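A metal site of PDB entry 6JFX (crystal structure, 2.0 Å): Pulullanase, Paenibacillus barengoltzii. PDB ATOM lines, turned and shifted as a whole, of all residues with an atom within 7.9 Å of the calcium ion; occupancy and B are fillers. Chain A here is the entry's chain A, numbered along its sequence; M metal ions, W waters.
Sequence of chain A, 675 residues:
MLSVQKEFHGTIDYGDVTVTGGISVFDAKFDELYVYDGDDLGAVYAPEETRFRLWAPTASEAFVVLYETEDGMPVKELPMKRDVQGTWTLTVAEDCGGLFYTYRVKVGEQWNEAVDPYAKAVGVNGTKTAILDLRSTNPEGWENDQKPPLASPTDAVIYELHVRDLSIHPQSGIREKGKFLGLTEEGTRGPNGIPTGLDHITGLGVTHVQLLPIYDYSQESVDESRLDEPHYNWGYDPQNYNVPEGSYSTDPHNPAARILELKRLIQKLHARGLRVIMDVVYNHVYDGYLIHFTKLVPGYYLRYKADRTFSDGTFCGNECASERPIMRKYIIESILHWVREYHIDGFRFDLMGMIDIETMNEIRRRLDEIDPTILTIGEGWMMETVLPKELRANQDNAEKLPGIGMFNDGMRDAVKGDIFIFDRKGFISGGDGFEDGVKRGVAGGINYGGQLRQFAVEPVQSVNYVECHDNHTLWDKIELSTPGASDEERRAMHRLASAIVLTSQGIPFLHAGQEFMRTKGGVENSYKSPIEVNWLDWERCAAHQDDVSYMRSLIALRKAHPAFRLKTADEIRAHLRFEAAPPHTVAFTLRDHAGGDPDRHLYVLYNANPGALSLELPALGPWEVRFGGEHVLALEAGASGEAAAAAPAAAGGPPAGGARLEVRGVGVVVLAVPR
The backbone NH (N) of Asn 125 lies within hydrogen-bond range of the side-chain carboxylate (OE1) of Glu 224 (2.9 Å).
OE2 of Glu 245 is in hydrogen-bond range of OG of Ser 247 (2.7 Å).
The side-chain carboxylate of Glu 224 is in salt-bridge range of the guanidinium group of Arg 258 (3.2 Å).
The side-chain hydroxyl of Tyr 217 is in hydrogen-bond range of the side-chain hydroxyl of Tyr 248 (2.8 Å).
ND2 of Asn 240 sits at hydrogen-bond distance from OD2 of Asp 216.
The backbone NH of Gln 239 lies within hydrogen-bond range of the backbone carbonyl oxygen of Asp 216 (2.9 Å).
The backbone NH (N) of Asp 216 sits at hydrogen-bond distance from the backbone carbonyl oxygen (O) of Val 243 (2.9 Å).
OE2 of Glu 224 lies close to N of Gly 246, at 3.0 Å.
The nearest printed residue that does not touch the calcium ion is Gly 246 (4.4 Å).
The calcium ion is bound by the side-chain carboxylate (OD1) of Asp 216 (2.2 Å), the backbone carbonyl oxygen (O) of Tyr 217 (2.2 Å), water W1 (2.2 Å), water W2 (2.3 Å), the side-chain carboxylate (OE2) of Glu 224 (2.3 Å) and the side-chain carboxylate (OE1) of Glu 245 (2.3 Å).
Water W1 lies within hydrogen-bond range of the side-chain carboxylate (OE2) of Glu 245 (2.6 Å) and the backbone carbonyl oxygen (O) of Val 222 (2.8 Å).
Water W2 lies within hydrogen-bond range of OD1 of Asn 125 (3.1 Å), OE1 of Gln 239 (3.4 Å) and N of Gln 219 (3.4 Å).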
ATOM      1  N   VAL A 122     -12.436   2.683 -24.291  1.00  0.00           N
ATOM      2  CA  VAL A 122     -11.017   2.912 -24.498  1.00  0.00           C
ATOM      3  C   VAL A 122     -10.234   2.393 -23.298  1.00  0.00           C
ATOM      4  O   VAL A 122     -10.766   2.209 -22.207  1.00  0.00           O
ATOM      5  CB  VAL A 122     -10.653   4.400 -24.726  1.00  0.00           C
ATOM      6  CG1 VAL A 122     -11.279   4.927 -26.001  1.00  0.00           C
ATOM      7  CG2 VAL A 122     -11.056   5.244 -23.484  1.00  0.00           C
ATOM      8  N   GLY A 123      -8.934   2.156 -23.518  1.00  0.00           N
ATOM      9  CA  GLY A 123      -8.020   1.881 -22.439  1.00  0.00           C
ATOM     10  C   GLY A 123      -7.660   3.144 -21.671  1.00  0.00           C
ATOM     11  O   GLY A 123      -8.103   4.253 -21.985  1.00  0.00           O
ATOM     12  N   VAL A 124      -6.826   2.965 -20.638  1.00  0.00           N
ATOM     13  CA  VAL A 124      -6.418   4.093 -19.818  1.00  0.00           C
ATOM     14  C   VAL A 124      -5.837   5.202 -20.696  1.00  0.00           C
ATOM     15  O   VAL A 124      -5.072   4.937 -21.633  1.00  0.00           O
ATOM     16  CB  VAL A 124      -5.413   3.631 -18.738  1.00  0.00           C
ATOM     17  CG1 VAL A 124      -4.058   3.280 -19.357  1.00  0.00           C
ATOM     18  CG2 VAL A 124      -5.246   4.705 -17.669  1.00  0.00           C
ATOM     19  N   ASN A 125      -6.244   6.448 -20.415  1.00  0.00           N
ATOM     20  CA  ASN A 125      -5.821   7.620 -21.166  1.00  0.00           C
ATOM     21  C   ASN A 125      -6.227   7.592 -22.637  1.00  0.00           C
ATOM     22  O   ASN A 125      -5.726   8.396 -23.424  1.00  0.00           O
ATOM     23  CB  ASN A 125      -4.321   7.846 -21.052  1.00  0.00           C
ATOM     24  CG  ASN A 125      -3.948   8.591 -19.794  1.00  0.00           C
ATOM     25  OD1 ASN A 125      -4.683   9.479 -19.355  1.00  0.00           O
ATOM     26  ND2 ASN A 125      -2.815   8.230 -19.199  1.00  0.00           N
ATOM     27  N   GLY A 126      -7.113   6.671 -23.027  1.00  0.00           N
ATOM     28  CA  GLY A 126      -7.767   6.725 -24.321  1.00  0.00           C
ATOM     29  C   GLY A 126      -6.863   6.623 -25.535  1.00  0.00           C
ATOM     30  O   GLY A 126      -7.157   7.242 -26.569  1.00  0.00           O
ATOM     31  N   TYR A 215     -17.169  13.480 -20.992  1.00  0.00           N
ATOM     32  CA  TYR A 215     -16.511  12.742 -22.059  1.00  0.00           C
ATOM     33  C   TYR A 215     -15.018  12.650 -21.742  1.00  0.00           C
ATOM     34  O   TYR A 215     -14.514  13.343 -20.854  1.00  0.00           O
ATOM     35  CB  TYR A 215     -16.734  13.425 -23.413  1.00  0.00           C
ATOM     36  CG  TYR A 215     -16.232  14.852 -23.364  1.00  0.00           C
ATOM     37  CD1 TYR A 215     -14.884  15.138 -23.526  1.00  0.00           C
ATOM     38  CD2 TYR A 215     -17.110  15.908 -23.078  1.00  0.00           C
ATOM     39  CE1 TYR A 215     -14.413  16.428 -23.431  1.00  0.00           C
ATOM     40  CE2 TYR A 215     -16.633  17.210 -22.985  1.00  0.00           C
ATOM     41  CZ  TYR A 215     -15.282  17.455 -23.149  1.00  0.00           C
ATOM     42  OH  TYR A 215     -14.775  18.735 -23.055  1.00  0.00           O
ATOM     43  N   ASP A 216     -14.300  11.850 -22.521  1.00  0.00           N
ATOM     44  CA  ASP A 216     -12.880  11.612 -22.255  1.00  0.00           C
ATOM     45  C   ASP A 216     -12.054  12.818 -22.722  1.00  0.00           C
ATOM     46  O   ASP A 216     -11.954  13.087 -23.927  1.00  0.00           O
ATOM     47  CB  ASP A 216     -12.408  10.344 -22.939  1.00  0.00           C
ATOM     48  CG  ASP A 216     -10.943  10.019 -22.626  1.00  0.00           C
ATOM     49  OD1 ASP A 216     -10.448  10.484 -21.585  1.00  0.00           O
ATOM     50  OD2 ASP A 216     -10.322   9.291 -23.400  1.00  0.00           O
ATOM     51  N   TYR A 217     -11.469  13.542 -21.779  1.00  0.00           N
ATOM     52  CA  TYR A 217     -10.592  14.644 -22.128  1.00  0.00           C
ATOM     53  C   TYR A 217      -9.131  14.232 -21.945  1.00  0.00           C
ATOM     54  O   TYR A 217      -8.826  13.134 -21.461  1.00  0.00           O
ATOM     55  CB  TYR A 217     -10.946  15.897 -21.311  1.00  0.00           C
ATOM     56  CG  TYR A 217     -11.031  15.758 -19.807  1.00  0.00           C
ATOM     57  CD1 TYR A 217      -9.883  15.821 -19.018  1.00  0.00           C
ATOM     58  CD2 TYR A 217     -12.276  15.648 -19.153  1.00  0.00           C
ATOM     59  CE1 TYR A 217      -9.945  15.741 -17.633  1.00  0.00           C
ATOM     60  CE2 TYR A 217     -12.353  15.567 -17.766  1.00  0.00           C
ATOM     61  CZ  TYR A 217     -11.184  15.616 -17.012  1.00  0.00           C
ATOM     62  OH  TYR A 217     -11.241  15.539 -15.639  1.00  0.00           O
ATOM     63  N   SER A 218      -8.225  15.100 -22.383  1.00  0.00           N
ATOM     64  CA  SER A 218      -6.877  14.632 -22.721  1.00  0.00           C
ATOM     65  C   SER A 218      -6.032  14.284 -21.503  1.00  0.00           C
ATOM     66  O   SER A 218      -6.206  14.830 -20.408  1.00  0.00           O
ATOM     67  CB  SER A 218      -6.146  15.702 -23.529  1.00  0.00           C
ATOM     68  OG  SER A 218      -5.638  16.670 -22.647  1.00  0.00           O
ATOM     69  N   GLN A 219      -5.062  13.397 -21.731  1.00  0.00           N
ATOM     70  CA  GLN A 219      -4.113  13.007 -20.683  1.00  0.00           C
ATOM     71  C   GLN A 219      -3.299  14.194 -20.176  1.00  0.00           C
ATOM     72  O   GLN A 219      -2.895  14.220 -19.014  1.00  0.00           O
ATOM     73  CB  GLN A 219      -3.183  11.919 -21.243  1.00  0.00           C
ATOM     74  CG  GLN A 219      -1.877  11.718 -20.490  1.00  0.00           C
ATOM     75  CD  GLN A 219      -1.081  10.541 -21.025  1.00  0.00           C
ATOM     76  OE1 GLN A 219      -1.390  10.004 -22.100  1.00  0.00           O
ATOM     77  NE2 GLN A 219      -0.062  10.128 -20.288  1.00  0.00           N
ATOM     78  N   GLU A 220      -3.073  15.210 -21.032  1.00  0.00           N
ATOM     79  CA  GLU A 220      -2.335  16.383 -20.605  1.00  0.00           C
ATOM     80  C   GLU A 220      -3.111  17.186 -19.555  1.00  0.00           C
ATOM     81  O   GLU A 220      -2.504  17.933 -18.773  1.00  0.00           O
ATOM     82  CB  GLU A 220      -1.999  17.273 -21.821  1.00  0.00           C
ATOM     83  CG  GLU A 220      -3.036  18.366 -22.110  1.00  0.00           C
ATOM     84  CD  GLU A 220      -3.067  18.813 -23.581  1.00  0.00           C
ATOM     85  OE1 GLU A 220      -2.106  19.479 -24.030  1.00  0.00           O
ATOM     86  OE2 GLU A 220      -4.073  18.520 -24.273  1.00  0.00           O
ATOM     87  N   SER A 221      -4.442  17.040 -19.525  1.00  0.00           N
ATOM     88  CA  SER A 221      -5.259  17.726 -18.542  1.00  0.00           C
ATOM     89  C   SER A 221      -5.269  16.969 -17.222  1.00  0.00           C
ATOM     90  O   SER A 221      -4.986  17.556 -16.163  1.00  0.00           O
ATOM     91  CB  SER A 221      -6.699  17.875 -19.059  1.00  0.00           C
ATOM     92  OG  SER A 221      -6.702  18.376 -20.380  1.00  0.00           O
ATOM     93  N   VAL A 222      -5.631  15.696 -17.268  1.00  0.00           N
ATOM     94  CA  VAL A 222      -5.538  14.801 -16.121  1.00  0.00           C
ATOM     95  C   VAL A 222      -4.952  13.492 -16.640  1.00  0.00           C
ATOM     96  O   VAL A 222      -5.495  12.898 -17.576  1.00  0.00           O
ATOM     97  CB  VAL A 222      -6.899  14.537 -15.443  1.00  0.00           C
ATOM     98  CG1 VAL A 222      -6.770  13.467 -14.350  1.00  0.00           C
ATOM     99  CG2 VAL A 222      -7.471  15.835 -14.848  1.00  0.00           C
ATOM    100  N   ASP A 223      -3.824  13.075 -16.061  1.00  0.00           N
ATOM    101  CA  ASP A 223      -3.207  11.797 -16.411  1.00  0.00           C
ATOM    102  C   ASP A 223      -3.926  10.680 -15.675  1.00  0.00           C
ATOM    103  O   ASP A 223      -3.783  10.541 -14.448  1.00  0.00           O
ATOM    104  CB  ASP A 223      -1.719  11.823 -16.066  1.00  0.00           C
ATOM    105  CG  ASP A 223      -0.970  10.606 -16.594  1.00  0.00           C
ATOM    106  OD1 ASP A 223      -1.606   9.549 -16.795  1.00  0.00           O
ATOM    107  OD2 ASP A 223       0.250  10.716 -16.816  1.00  0.00           O
ATOM    108  N   GLU A 224      -4.703   9.872 -16.410  1.00  0.00           N
ATOM    109  CA  GLU A 224      -5.505   8.838 -15.765  1.00  0.00           C
ATOM    110  C   GLU A 224      -4.671   7.720 -15.168  1.00  0.00           C
ATOM    111  O   GLU A 224      -5.225   6.867 -14.459  1.00  0.00           O
ATOM    112  CB  GLU A 224      -6.505   8.224 -16.750  1.00  0.00           C
ATOM    113  CG  GLU A 224      -7.435   9.231 -17.398  1.00  0.00           C
ATOM    114  CD  GLU A 224      -8.344   8.590 -18.427  1.00  0.00           C
ATOM    115  OE1 GLU A 224      -8.283   7.350 -18.574  1.00  0.00           O
ATOM    116  OE2 GLU A 224      -9.128   9.303 -19.083  1.00  0.00           O
ATOM    117  N   ASP A 237     -10.852  19.866 -23.026  1.00  0.00           N
ATOM    118  CA  ASP A 237      -9.816  19.450 -23.977  1.00  0.00           C
ATOM    119  C   ASP A 237     -10.199  18.066 -24.499  1.00  0.00           C
ATOM    120  O   ASP A 237      -9.647  17.056 -24.057  1.00  0.00           O
ATOM    121  CB  ASP A 237      -8.442  19.410 -23.310  1.00  0.00           C
ATOM    122  CG  ASP A 237      -8.177  20.625 -22.414  1.00  0.00           C
ATOM    123  OD1 ASP A 237      -8.168  21.761 -22.947  1.00  0.00           O
ATOM    124  OD2 ASP A 237      -7.962  20.457 -21.200  1.00  0.00           O
ATOM    125  N   GLN A 239     -10.737  14.508 -26.206  1.00  0.00           N
ATOM    126  CA  GLN A 239      -9.940  13.486 -26.886  1.00  0.00           C
ATOM    127  C   GLN A 239     -10.795  12.385 -27.486  1.00  0.00           C
ATOM    128  O   GLN A 239     -10.637  12.079 -28.687  1.00  0.00           O
ATOM    129  CB  GLN A 239      -8.919  12.893 -25.898  1.00  0.00           C
ATOM    130  CG  GLN A 239      -7.891  11.934 -26.553  1.00  0.00           C
ATOM    131  CD  GLN A 239      -7.082  11.184 -25.499  1.00  0.00           C
ATOM    132  OE1 GLN A 239      -7.122  11.518 -24.315  1.00  0.00           O
ATOM    133  NE2 GLN A 239      -6.352  10.157 -25.929  1.00  0.00           N
ATOM    134  N   ASN A 240     -11.709  11.778 -26.733  1.00  0.00           N
ATOM    135  CA  ASN A 240     -12.629  10.775 -27.258  1.00  0.00           C
ATOM    136  C   ASN A 240     -14.058  11.189 -26.908  1.00  0.00           C
ATOM    137  O   ASN A 240     -14.464  11.112 -25.744  1.00  0.00           O
ATOM    138  CB  ASN A 240     -12.301   9.371 -26.731  1.00  0.00           C
ATOM    139  CG  ASN A 240     -10.901   8.918 -27.121  1.00  0.00           C
ATOM    140  OD1 ASN A 240     -10.601   8.743 -28.298  1.00  0.00           O
ATOM    141  ND2 ASN A 240     -10.022   8.759 -26.134  1.00  0.00           N
ATOM    142  N   VAL A 243     -16.903   8.355 -25.289  1.00  0.00           N
ATOM    143  CA  VAL A 243     -16.579   7.513 -24.146  1.00  0.00           C
ATOM    144  C   VAL A 243     -16.403   8.406 -22.920  1.00  0.00           C
ATOM    145  O   VAL A 243     -16.019   9.573 -23.045  1.00  0.00           O
ATOM    146  CB  VAL A 243     -15.332   6.663 -24.450  1.00  0.00           C
ATOM    147  CG1 VAL A 243     -14.094   7.517 -24.448  1.00  0.00           C
ATOM    148  CG2 VAL A 243     -15.178   5.493 -23.476  1.00  0.00           C
ATOM    149  N   PRO A 244     -16.731   7.914 -21.723  1.00  0.00           N
ATOM    150  CA  PRO A 244     -16.583   8.760 -20.530  1.00  0.00           C
ATOM    151  C   PRO A 244     -15.123   9.024 -20.168  1.00  0.00           C
ATOM    152  O   PRO A 244     -14.212   8.299 -20.583  1.00  0.00           O
ATOM    153  CB  PRO A 244     -17.273   7.958 -19.422  1.00  0.00           C
ATOM    154  CG  PRO A 244     -18.241   7.038 -20.150  1.00  0.00           C
ATOM    155  CD  PRO A 244     -17.504   6.692 -21.420  1.00  0.00           C
ATOM    156  N   GLU A 245     -14.926  10.076 -19.372  1.00  0.00           N
ATOM    157  CA  GLU A 245     -13.597  10.383 -18.819  1.00  0.00           C
ATOM    158  C   GLU A 245     -13.157   9.322 -17.824  1.00  0.00           C
ATOM    159  O   GLU A 245     -13.910   8.944 -16.907  1.00  0.00           O
ATOM    160  CB  GLU A 245     -13.623  11.773 -18.155  1.00  0.00           C
ATOM    161  CG  GLU A 245     -12.472  12.046 -17.155  1.00  0.00           C
ATOM    162  CD  GLU A 245     -11.091  11.951 -17.774  1.00  0.00           C
ATOM    163  OE1 GLU A 245     -10.957  11.976 -19.019  1.00  0.00           O
ATOM    164  OE2 GLU A 245     -10.109  11.831 -17.002  1.00  0.00           O
ATOM    165  N   GLY A 246     -11.910   8.865 -17.982  1.00  0.00           N
ATOM    166  CA  GLY A 246     -11.423   7.746 -17.182  1.00  0.00           C
ATOM    167  C   GLY A 246     -11.195   8.106 -15.717  1.00  0.00           C
ATOM    168  O   GLY A 246     -11.381   7.256 -14.829  1.00  0.00           O
ATOM    169  N   SER A 247     -10.763   9.330 -15.432  1.00  0.00           N
ATOM    170  CA  SER A 247     -10.433   9.668 -14.053  1.00  0.00           C
ATOM    171  C   SER A 247     -11.671   9.731 -13.155  1.00  0.00           C
ATOM    172  O   SER A 247     -11.522   9.717 -11.925  1.00  0.00           O
ATOM    173  CB  SER A 247      -9.659  10.982 -13.975  1.00  0.00           C
ATOM    174  OG  SER A 247     -10.461  12.103 -14.330  1.00  0.00           O
ATOM    175  N   TYR A 248     -12.873   9.766 -13.718  1.00  0.00           N
ATOM    176  CA  TYR A 248     -14.068   9.742 -12.896  1.00  0.00           C
ATOM    177  C   TYR A 248     -14.552   8.331 -12.593  1.00  0.00           C
ATOM    178  O   TYR A 248     -15.595   8.177 -11.942  1.00  0.00           O
ATOM    179  CB  TYR A 248     -15.172  10.563 -13.565  1.00  0.00           C
ATOM    180  CG  TYR A 248     -14.801  12.030 -13.802  1.00  0.00           C
ATOM    181  CD1 TYR A 248     -13.913  12.680 -12.959  1.00  0.00           C
ATOM    182  CD2 TYR A 248     -15.324  12.732 -14.876  1.00  0.00           C
ATOM    183  CE1 TYR A 248     -13.560  14.016 -13.175  1.00  0.00           C
ATOM    184  CE2 TYR A 248     -14.973  14.074 -15.117  1.00  0.00           C
ATOM    185  CZ  TYR A 248     -14.097  14.708 -14.259  1.00  0.00           C
ATOM    186  OH  TYR A 248     -13.738  16.021 -14.503  1.00  0.00           O
ATOM    187  N   ARG A 258     -15.780   2.839 -16.279  1.00  0.00           N
ATOM    188  CA  ARG A 258     -16.292   4.200 -16.446  1.00  0.00           C
ATOM    189  C   ARG A 258     -17.677   4.217 -17.093  1.00  0.00           C
ATOM    190  O   ARG A 258     -18.486   5.090 -16.798  1.00  0.00           O
ATOM    191  CB  ARG A 258     -15.297   5.021 -17.257  1.00  0.00           C
ATOM    192  CG  ARG A 258     -15.106   4.493 -18.686  1.00  0.00           C
ATOM    193  CD  ARG A 258     -14.069   5.285 -19.444  1.00  0.00           C
ATOM    194  NE  ARG A 258     -12.704   4.895 -19.100  1.00  0.00           N
ATOM    195  CZ  ARG A 258     -11.628   5.454 -19.627  1.00  0.00           C
ATOM    196  NH1 ARG A 258     -11.750   6.448 -20.503  1.00  0.00           N
ATOM    197  NH2 ARG A 258     -10.417   5.037 -19.275  1.00  0.00           N
HETATM  198 CA    CA M   1      -9.017  11.332 -20.136  1.00  0.00          CA
HETATM  199  O   HOH W   1      -8.090  12.478 -18.439  1.00  0.00           O
HETATM  200  O   HOH W   2      -7.026  10.719 -21.026  1.00  0.00           O
